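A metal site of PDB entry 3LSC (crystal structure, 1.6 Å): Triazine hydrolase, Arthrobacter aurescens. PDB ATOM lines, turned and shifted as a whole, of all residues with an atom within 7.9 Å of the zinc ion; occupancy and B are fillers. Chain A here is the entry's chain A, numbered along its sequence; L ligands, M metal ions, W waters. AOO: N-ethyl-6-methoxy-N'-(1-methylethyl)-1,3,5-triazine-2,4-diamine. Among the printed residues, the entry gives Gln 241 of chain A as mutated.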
ATOM      1  N   HIS A  63     -15.696 -22.091 -20.742  1.00  0.00           N
ATOM      2  CA  HIS A  63     -14.630 -21.295 -20.108  1.00  0.00           C
ATOM      3  C   HIS A  63     -14.504 -21.574 -18.603  1.00  0.00           C
ATOM      4  O   HIS A  63     -15.344 -21.126 -17.811  1.00  0.00           O
ATOM      5  CB  HIS A  63     -14.866 -19.802 -20.370  1.00  0.00           C
ATOM      6  CG  HIS A  63     -13.702 -18.917 -19.985  1.00  0.00           C
ATOM      7  ND1 HIS A  63     -12.591 -18.761 -20.771  1.00  0.00           N
ATOM      8  CD2 HIS A  63     -13.526 -18.115 -18.907  1.00  0.00           C
ATOM      9  CE1 HIS A  63     -11.750 -17.914 -20.189  1.00  0.00           C
ATOM     10  NE2 HIS A  63     -12.302 -17.503 -19.061  1.00  0.00           N
ATOM     11  N   GLN A  64     -13.469 -22.326 -18.234  1.00  0.00           N
ATOM     12  CA  GLN A  64     -13.112 -22.592 -16.843  1.00  0.00           C
ATOM     13  C   GLN A  64     -11.689 -22.104 -16.508  1.00  0.00           C
ATOM     14  O   GLN A  64     -10.878 -21.872 -17.402  1.00  0.00           O
ATOM     15  CB  GLN A  64     -13.209 -24.097 -16.534  1.00  0.00           C
ATOM     16  CG  GLN A  64     -14.466 -24.539 -15.800  1.00  0.00           C
ATOM     17  CD  GLN A  64     -14.486 -24.128 -14.340  1.00  0.00           C
ATOM     18  OE1 GLN A  64     -13.572 -23.448 -13.854  1.00  0.00           O
ATOM     19  NE2 GLN A  64     -15.539 -24.527 -13.624  1.00  0.00           N
ATOM     20  N   HIS A  65     -11.426 -21.930 -15.220  1.00  0.00           N
ATOM     21  CA  HIS A  65     -10.060 -21.852 -14.692  1.00  0.00           C
ATOM     22  C   HIS A  65     -10.061 -22.785 -13.480  1.00  0.00           C
ATOM     23  O   HIS A  65     -10.327 -22.375 -12.339  1.00  0.00           O
ATOM     24  CB  HIS A  65      -9.695 -20.441 -14.241  1.00  0.00           C
ATOM     25  CG  HIS A  65      -9.818 -19.415 -15.330  1.00  0.00           C
ATOM     26  ND1 HIS A  65      -9.164 -19.538 -16.532  1.00  0.00           N
ATOM     27  CD2 HIS A  65     -10.500 -18.247 -15.382  1.00  0.00           C
ATOM     28  CE1 HIS A  65      -9.438 -18.491 -17.293  1.00  0.00           C
ATOM     29  NE2 HIS A  65     -10.245 -17.692 -16.617  1.00  0.00           N
ATOM     30  N   GLU A  68      -8.599 -22.404  -9.802  1.00  0.00           N
ATOM     31  CA  GLU A  68      -9.285 -21.481  -8.889  1.00  0.00           C
ATOM     32  C   GLU A  68     -10.266 -22.143  -7.905  1.00  0.00           C
ATOM     33  O   GLU A  68     -10.790 -21.491  -7.010  1.00  0.00           O
ATOM     34  CB  GLU A  68      -9.991 -20.366  -9.655  1.00  0.00           C
ATOM     35  CG  GLU A  68      -9.047 -19.481 -10.463  1.00  0.00           C
ATOM     36  CD  GLU A  68      -9.764 -18.370 -11.210  1.00  0.00           C
ATOM     37  OE1 GLU A  68     -11.000 -18.242 -11.066  1.00  0.00           O
ATOM     38  OE2 GLU A  68      -9.069 -17.633 -11.934  1.00  0.00           O
ATOM     39  N   MET A  82     -11.771  -5.502 -10.409  1.00  0.00           N
ATOM     40  CA  MET A  82     -10.868  -6.394 -11.141  1.00  0.00           C
ATOM     41  C   MET A  82      -9.397  -6.294 -10.737  1.00  0.00           C
ATOM     42  O   MET A  82      -8.727  -7.320 -10.566  1.00  0.00           O
ATOM     43  CB  MET A  82     -11.007  -6.158 -12.653  1.00  0.00           C
ATOM     44  CG  MET A  82     -10.079  -7.054 -13.467  1.00  0.00           C
ATOM     45  SD  MET A  82     -10.430  -8.779 -13.104  1.00  0.00           S
ATOM     46  CE  MET A  82      -9.451  -9.580 -14.384  1.00  0.00           C
ATOM     47  N   TRP A  85      -8.698  -7.847  -7.465  1.00  0.00           N
ATOM     48  CA  TRP A  85      -8.963  -9.272  -7.587  1.00  0.00           C
ATOM     49  C   TRP A  85      -7.813 -10.009  -8.245  1.00  0.00           C
ATOM     50  O   TRP A  85      -7.350 -11.030  -7.729  1.00  0.00           O
ATOM     51  CB  TRP A  85     -10.249  -9.488  -8.388  1.00  0.00           C
ATOM     52  CG  TRP A  85     -10.629 -10.929  -8.531  1.00  0.00           C
ATOM     53  CD1 TRP A  85     -11.446 -11.644  -7.708  1.00  0.00           C
ATOM     54  CD2 TRP A  85     -10.215 -11.823  -9.568  1.00  0.00           C
ATOM     55  NE1 TRP A  85     -11.556 -12.936  -8.167  1.00  0.00           N
ATOM     56  CE2 TRP A  85     -10.809 -13.071  -9.305  1.00  0.00           C
ATOM     57  CE3 TRP A  85      -9.385 -11.686 -10.703  1.00  0.00           C
ATOM     58  CZ2 TRP A  85     -10.622 -14.180 -10.137  1.00  0.00           C
ATOM     59  CZ3 TRP A  85      -9.187 -12.790 -11.516  1.00  0.00           C
ATOM     60  CH2 TRP A  85      -9.802 -14.018 -11.224  1.00  0.00           C
ATOM     61  N   GLN A 129      -8.839 -23.031 -19.138  1.00  0.00           N
ATOM     62  CA  GLN A 129      -7.759 -22.144 -19.562  1.00  0.00           C
ATOM     63  C   GLN A 129      -6.813 -21.932 -18.386  1.00  0.00           C
ATOM     64  O   GLN A 129      -7.109 -21.167 -17.453  1.00  0.00           O
ATOM     65  CB  GLN A 129      -8.325 -20.816 -20.071  1.00  0.00           C
ATOM     66  CG  GLN A 129      -7.274 -19.881 -20.678  1.00  0.00           C
ATOM     67  CD  GLN A 129      -7.837 -18.522 -21.022  1.00  0.00           C
ATOM     68  OE1 GLN A 129      -8.726 -18.004 -20.346  1.00  0.00           O
ATOM     69  NE2 GLN A 129      -7.319 -17.923 -22.100  1.00  0.00           N
ATOM     70  N   LEU A 131      -3.224 -20.711 -17.017  1.00  0.00           N
ATOM     71  CA  LEU A 131      -2.074 -19.839 -17.317  1.00  0.00           C
ATOM     72  C   LEU A 131      -0.942 -19.903 -16.277  1.00  0.00           C
ATOM     73  O   LEU A 131       0.117 -19.306 -16.486  1.00  0.00           O
ATOM     74  CB  LEU A 131      -2.524 -18.386 -17.483  1.00  0.00           C
ATOM     75  CG  LEU A 131      -3.189 -17.689 -16.285  1.00  0.00           C
ATOM     76  CD1 LEU A 131      -2.180 -17.482 -15.154  1.00  0.00           C
ATOM     77  CD2 LEU A 131      -3.775 -16.359 -16.722  1.00  0.00           C
ATOM     78  N   CYS A 211      -3.931 -15.230 -22.346  1.00  0.00           N
ATOM     79  CA  CYS A 211      -4.817 -14.608 -21.368  1.00  0.00           C
ATOM     80  C   CYS A 211      -5.551 -13.417 -21.992  1.00  0.00           C
ATOM     81  O   CYS A 211      -6.748 -13.240 -21.789  1.00  0.00           O
ATOM     82  CB  CYS A 211      -4.036 -14.187 -20.132  1.00  0.00           C
ATOM     83  SG  CYS A 211      -5.156 -13.742 -18.792  1.00  0.00           S
ATOM     84  N   HIS A 236      -8.430 -19.230 -28.340  1.00  0.00           N
ATOM     85  CA  HIS A 236      -9.309 -18.768 -27.269  1.00  0.00           C
ATOM     86  C   HIS A 236      -8.626 -17.665 -26.476  1.00  0.00           C
ATOM     87  O   HIS A 236      -7.443 -17.762 -26.183  1.00  0.00           O
ATOM     88  CB  HIS A 236      -9.691 -19.939 -26.338  1.00  0.00           C
ATOM     89  CG  HIS A 236     -10.627 -19.558 -25.228  1.00  0.00           C
ATOM     90  ND1 HIS A 236     -11.806 -18.869 -25.437  1.00  0.00           N
ATOM     91  CD2 HIS A 236     -10.588 -19.826 -23.895  1.00  0.00           C
ATOM     92  CE1 HIS A 236     -12.429 -18.680 -24.285  1.00  0.00           C
ATOM     93  NE2 HIS A 236     -11.718 -19.268 -23.338  1.00  0.00           N
ATOM     94  N   THR A 237      -9.366 -16.620 -26.119  1.00  0.00           N
ATOM     95  CA  THR A 237      -8.815 -15.583 -25.242  1.00  0.00           C
ATOM     96  C   THR A 237      -9.933 -14.778 -24.597  1.00  0.00           C
ATOM     97  O   THR A 237     -11.097 -14.926 -24.971  1.00  0.00           O
ATOM     98  CB  THR A 237      -7.835 -14.643 -26.007  1.00  0.00           C
ATOM     99  OG1 THR A 237      -7.108 -13.840 -25.064  1.00  0.00           O
ATOM    100  CG2 THR A 237      -8.566 -13.735 -26.970  1.00  0.00           C
ATOM    101  N   HIS A 238      -9.598 -13.969 -23.590  1.00  0.00           N
ATOM    102  CA  HIS A 238     -10.551 -13.037 -23.001  1.00  0.00           C
ATOM    103  C   HIS A 238     -10.806 -11.861 -23.951  1.00  0.00           C
ATOM    104  O   HIS A 238      -9.954 -11.521 -24.766  1.00  0.00           O
ATOM    105  CB  HIS A 238     -10.050 -12.524 -21.655  1.00  0.00           C
ATOM    106  CG  HIS A 238      -9.959 -13.581 -20.603  1.00  0.00           C
ATOM    107  ND1 HIS A 238      -8.768 -14.172 -20.245  1.00  0.00           N
ATOM    108  CD2 HIS A 238     -10.921 -14.154 -19.833  1.00  0.00           C
ATOM    109  CE1 HIS A 238      -8.989 -15.055 -19.290  1.00  0.00           C
ATOM    110  NE2 HIS A 238     -10.284 -15.067 -19.028  1.00  0.00           N
ATOM    111  N   GLN A 241     -13.287  -7.203 -21.624  1.00  0.00           N
ATOM    112  CA  GLN A 241     -13.534  -6.911 -20.224  1.00  0.00           C
ATOM    113  C   GLN A 241     -13.378  -5.390 -20.105  1.00  0.00           C
ATOM    114  O   GLN A 241     -12.591  -4.789 -20.824  1.00  0.00           O
ATOM    115  CB  GLN A 241     -12.529  -7.638 -19.338  1.00  0.00           C
ATOM    116  CG  GLN A 241     -12.565  -9.164 -19.501  1.00  0.00           C
ATOM    117  CD  GLN A 241     -11.760  -9.905 -18.433  1.00  0.00           C
ATOM    118  OE1 GLN A 241     -12.077 -11.045 -18.075  1.00  0.00           O
ATOM    119  NE2 GLN A 241     -10.732  -9.249 -17.915  1.00  0.00           N
ATOM    120  N   ALA A 273     -14.014 -15.074 -24.631  1.00  0.00           N
ATOM    121  CA  ALA A 273     -14.688 -15.109 -23.329  1.00  0.00           C
ATOM    122  C   ALA A 273     -15.153 -13.726 -22.877  1.00  0.00           C
ATOM    123  O   ALA A 273     -14.398 -12.749 -22.960  1.00  0.00           O
ATOM    124  CB  ALA A 273     -13.731 -15.712 -22.280  1.00  0.00           C
ATOM    125  N   HIS A 274     -16.395 -13.653 -22.373  1.00  0.00           N
ATOM    126  CA  HIS A 274     -17.023 -12.430 -21.840  1.00  0.00           C
ATOM    127  C   HIS A 274     -17.645 -11.524 -22.905  1.00  0.00           C
ATOM    128  O   HIS A 274     -18.870 -11.445 -23.022  1.00  0.00           O
ATOM    129  CB  HIS A 274     -16.069 -11.610 -20.966  1.00  0.00           C
ATOM    130  CG  HIS A 274     -15.527 -12.339 -19.775  1.00  0.00           C
ATOM    131  ND1 HIS A 274     -16.239 -12.486 -18.597  1.00  0.00           N
ATOM    132  CD2 HIS A 274     -14.356 -12.991 -19.584  1.00  0.00           C
ATOM    133  CE1 HIS A 274     -15.516 -13.160 -17.726  1.00  0.00           C
ATOM    134  NE2 HIS A 274     -14.373 -13.496 -18.309  1.00  0.00           N
ATOM    135  N   LEU A 296     -20.523 -15.212 -19.996  1.00  0.00           N
ATOM    136  CA  LEU A 296     -20.143 -15.607 -18.647  1.00  0.00           C
ATOM    137  C   LEU A 296     -20.815 -14.676 -17.642  1.00  0.00           C
ATOM    138  O   LEU A 296     -20.182 -13.794 -17.057  1.00  0.00           O
ATOM    139  CB  LEU A 296     -18.614 -15.590 -18.475  1.00  0.00           C
ATOM    140  CG  LEU A 296     -17.791 -16.273 -19.586  1.00  0.00           C
ATOM    141  CD1 LEU A 296     -16.303 -15.992 -19.440  1.00  0.00           C
ATOM    142  CD2 LEU A 296     -18.046 -17.761 -19.570  1.00  0.00           C
ATOM    143  N   PRO A 299     -19.307 -14.072 -13.511  1.00  0.00           N
ATOM    144  CA  PRO A 299     -18.185 -13.146 -13.266  1.00  0.00           C
ATOM    145  C   PRO A 299     -18.491 -11.703 -13.730  1.00  0.00           C
ATOM    146  O   PRO A 299     -18.040 -10.745 -13.078  1.00  0.00           O
ATOM    147  CB  PRO A 299     -17.047 -13.739 -14.102  1.00  0.00           C
ATOM    148  CG  PRO A 299     -17.687 -14.626 -15.109  1.00  0.00           C
ATOM    149  CD  PRO A 299     -18.942 -15.159 -14.431  1.00  0.00           C
ATOM    150  N   TRP A 305     -19.292  -5.559 -13.814  1.00  0.00           N
ATOM    151  CA  TRP A 305     -19.128  -5.192 -15.221  1.00  0.00           C
ATOM    152  C   TRP A 305     -20.449  -4.959 -15.931  1.00  0.00           C
ATOM    153  O   TRP A 305     -20.567  -4.086 -16.769  1.00  0.00           O
ATOM    154  CB  TRP A 305     -18.344  -6.281 -15.955  1.00  0.00           C
ATOM    155  CG  TRP A 305     -16.924  -6.367 -15.512  1.00  0.00           C
ATOM    156  CD1 TRP A 305     -16.236  -5.444 -14.794  1.00  0.00           C
ATOM    157  CD2 TRP A 305     -16.007  -7.430 -15.786  1.00  0.00           C
ATOM    158  NE1 TRP A 305     -14.948  -5.863 -14.589  1.00  0.00           N
ATOM    159  CE2 TRP A 305     -14.777  -7.087 -15.184  1.00  0.00           C
ATOM    160  CE3 TRP A 305     -16.102  -8.646 -16.470  1.00  0.00           C
ATOM    161  CZ2 TRP A 305     -13.656  -7.904 -15.256  1.00  0.00           C
ATOM    162  CZ3 TRP A 305     -14.996  -9.461 -16.539  1.00  0.00           C
ATOM    163  CH2 TRP A 305     -13.775  -9.084 -15.930  1.00  0.00           C
ATOM    164  N   THR A 324     -18.750 -20.648 -16.964  1.00  0.00           N
ATOM    165  CA  THR A 324     -18.835 -20.189 -15.587  1.00  0.00           C
ATOM    166  C   THR A 324     -17.665 -19.306 -15.173  1.00  0.00           C
ATOM    167  O   THR A 324     -17.750 -18.580 -14.189  1.00  0.00           O
ATOM    168  CB  THR A 324     -18.835 -21.370 -14.603  1.00  0.00           C
ATOM    169  OG1 THR A 324     -17.627 -22.131 -14.760  1.00  0.00           O
ATOM    170  CG2 THR A 324     -20.058 -22.266 -14.825  1.00  0.00           C
ATOM    171  N   THR A 325     -16.570 -19.375 -15.947  1.00  0.00           N
ATOM    172  CA  THR A 325     -15.237 -18.956 -15.500  1.00  0.00           C
ATOM    173  C   THR A 325     -14.787 -19.747 -14.275  1.00  0.00           C
ATOM    174  O   THR A 325     -15.489 -20.649 -13.811  1.00  0.00           O
ATOM    175  CB  THR A 325     -15.064 -17.405 -15.317  1.00  0.00           C
ATOM    176  OG1 THR A 325     -13.680 -17.094 -15.519  1.00  0.00           O
ATOM    177  CG2 THR A 325     -15.457 -16.935 -13.921  1.00  0.00           C
ATOM    178  N   GLY A 326     -13.598 -19.409 -13.760  1.00  0.00           N
ATOM    179  CA  GLY A 326     -13.054 -20.097 -12.606  1.00  0.00           C
ATOM    180  C   GLY A 326     -13.752 -19.751 -11.293  1.00  0.00           C
ATOM    181  O   GLY A 326     -14.412 -18.716 -11.165  1.00  0.00           O
ATOM    182  N   SER A 329     -13.952 -16.338  -9.210  1.00  0.00           N
ATOM    183  CA  SER A 329     -14.839 -15.259  -9.663  1.00  0.00           C
ATOM    184  C   SER A 329     -16.183 -15.842 -10.064  1.00  0.00           C
ATOM    185  O   SER A 329     -16.689 -15.553 -11.152  1.00  0.00           O
ATOM    186  CB  SER A 329     -14.231 -14.508 -10.855  1.00  0.00           C
ATOM    187  OG  SER A 329     -15.088 -13.439 -11.236  1.00  0.00           O
HETATM  188  N1  AOO L   1     -10.978 -12.756 -15.529  1.00  0.00           N
HETATM  189  C2  AOO L   1     -11.456 -13.620 -14.660  1.00  0.00           C
HETATM  190  N3  AOO L   1     -10.711 -14.673 -14.234  1.00  0.00           N
HETATM  191  C4  AOO L   1      -9.435 -14.805 -14.721  1.00  0.00           C
HETATM  192  N5  AOO L   1      -8.939 -13.919 -15.585  1.00  0.00           N
HETATM  193  C6  AOO L   1      -9.666 -12.917 -16.008  1.00  0.00           C
HETATM  194  N7  AOO L   1      -8.506 -15.812 -14.339  1.00  0.00           N
HETATM  195  C8  AOO L   1      -7.141 -16.253 -14.336  1.00  0.00           C
HETATM  196  C9  AOO L   1      -6.907 -17.702 -14.065  1.00  0.00           C
HETATM  197  C10 AOO L   1      -6.287 -15.307 -13.567  1.00  0.00           C
HETATM  198  N11 AOO L   1      -9.031 -12.040 -16.927  1.00  0.00           N
HETATM  199  C12 AOO L   1      -7.875 -11.446 -17.515  1.00  0.00           C
HETATM  200  C13 AOO L   1      -6.705 -11.453 -16.594  1.00  0.00           C
HETATM  201  O21 AOO L   1     -12.749 -13.463 -14.192  1.00  0.00           O
HETATM  202  C22 AOO L   1     -13.494 -12.381 -14.627  1.00  0.00           C
HETATM  203 ZN    ZN M   1     -11.275 -16.276 -17.715  1.00  0.00          ZN
HETATM  204  O   HOH W   1     -12.601 -15.149 -16.752  1.00  0.00           O
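OE1 of Gln 241 sits close to N1 of the ligand (3.3 Å).
N7 of the ligand sits close to NE2 of His 65, 3.4 Å away.
The side-chain carboxylate (OE2) of Glu 68 sits close to a nitrogen (N7) of the ligand (3.1 Å).
O of His 63 lies within hydrogen-bond range of N of Thr 325, at 2.8 Å.
A ring nitrogen (ND1) of His 65 is in hydrogen-bond range of the backbone carbonyl oxygen of Gln 129 (2.8 Å).
The backbone carbonyl oxygen of Cys 211 lies within hydrogen-bond range of a ring nitrogen (ND1) of His 238 (2.7 Å).
OE1 of Gln 64 lies close to O of Thr 325 (3.4 Å).
A ring nitrogen (NE2) of His 236 is in hydrogen-bond range of a ring nitrogen (ND1) of His 63 (2.8 Å).
Thr 325 touches the zinc ion.
Of the 22 residues printed, 4 come within 4 Å of the zinc ion.
The zinc ion is bound by water W1, NE2 of His 238, NE2 of His 65 and NE2 of His 63.
Water W1 lies within hydrogen-bond range of OG1 of Thr 325 (2.5 Å), NE2 of His 274 (2.9 Å) and O21 of the ligand (3.1 Å).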
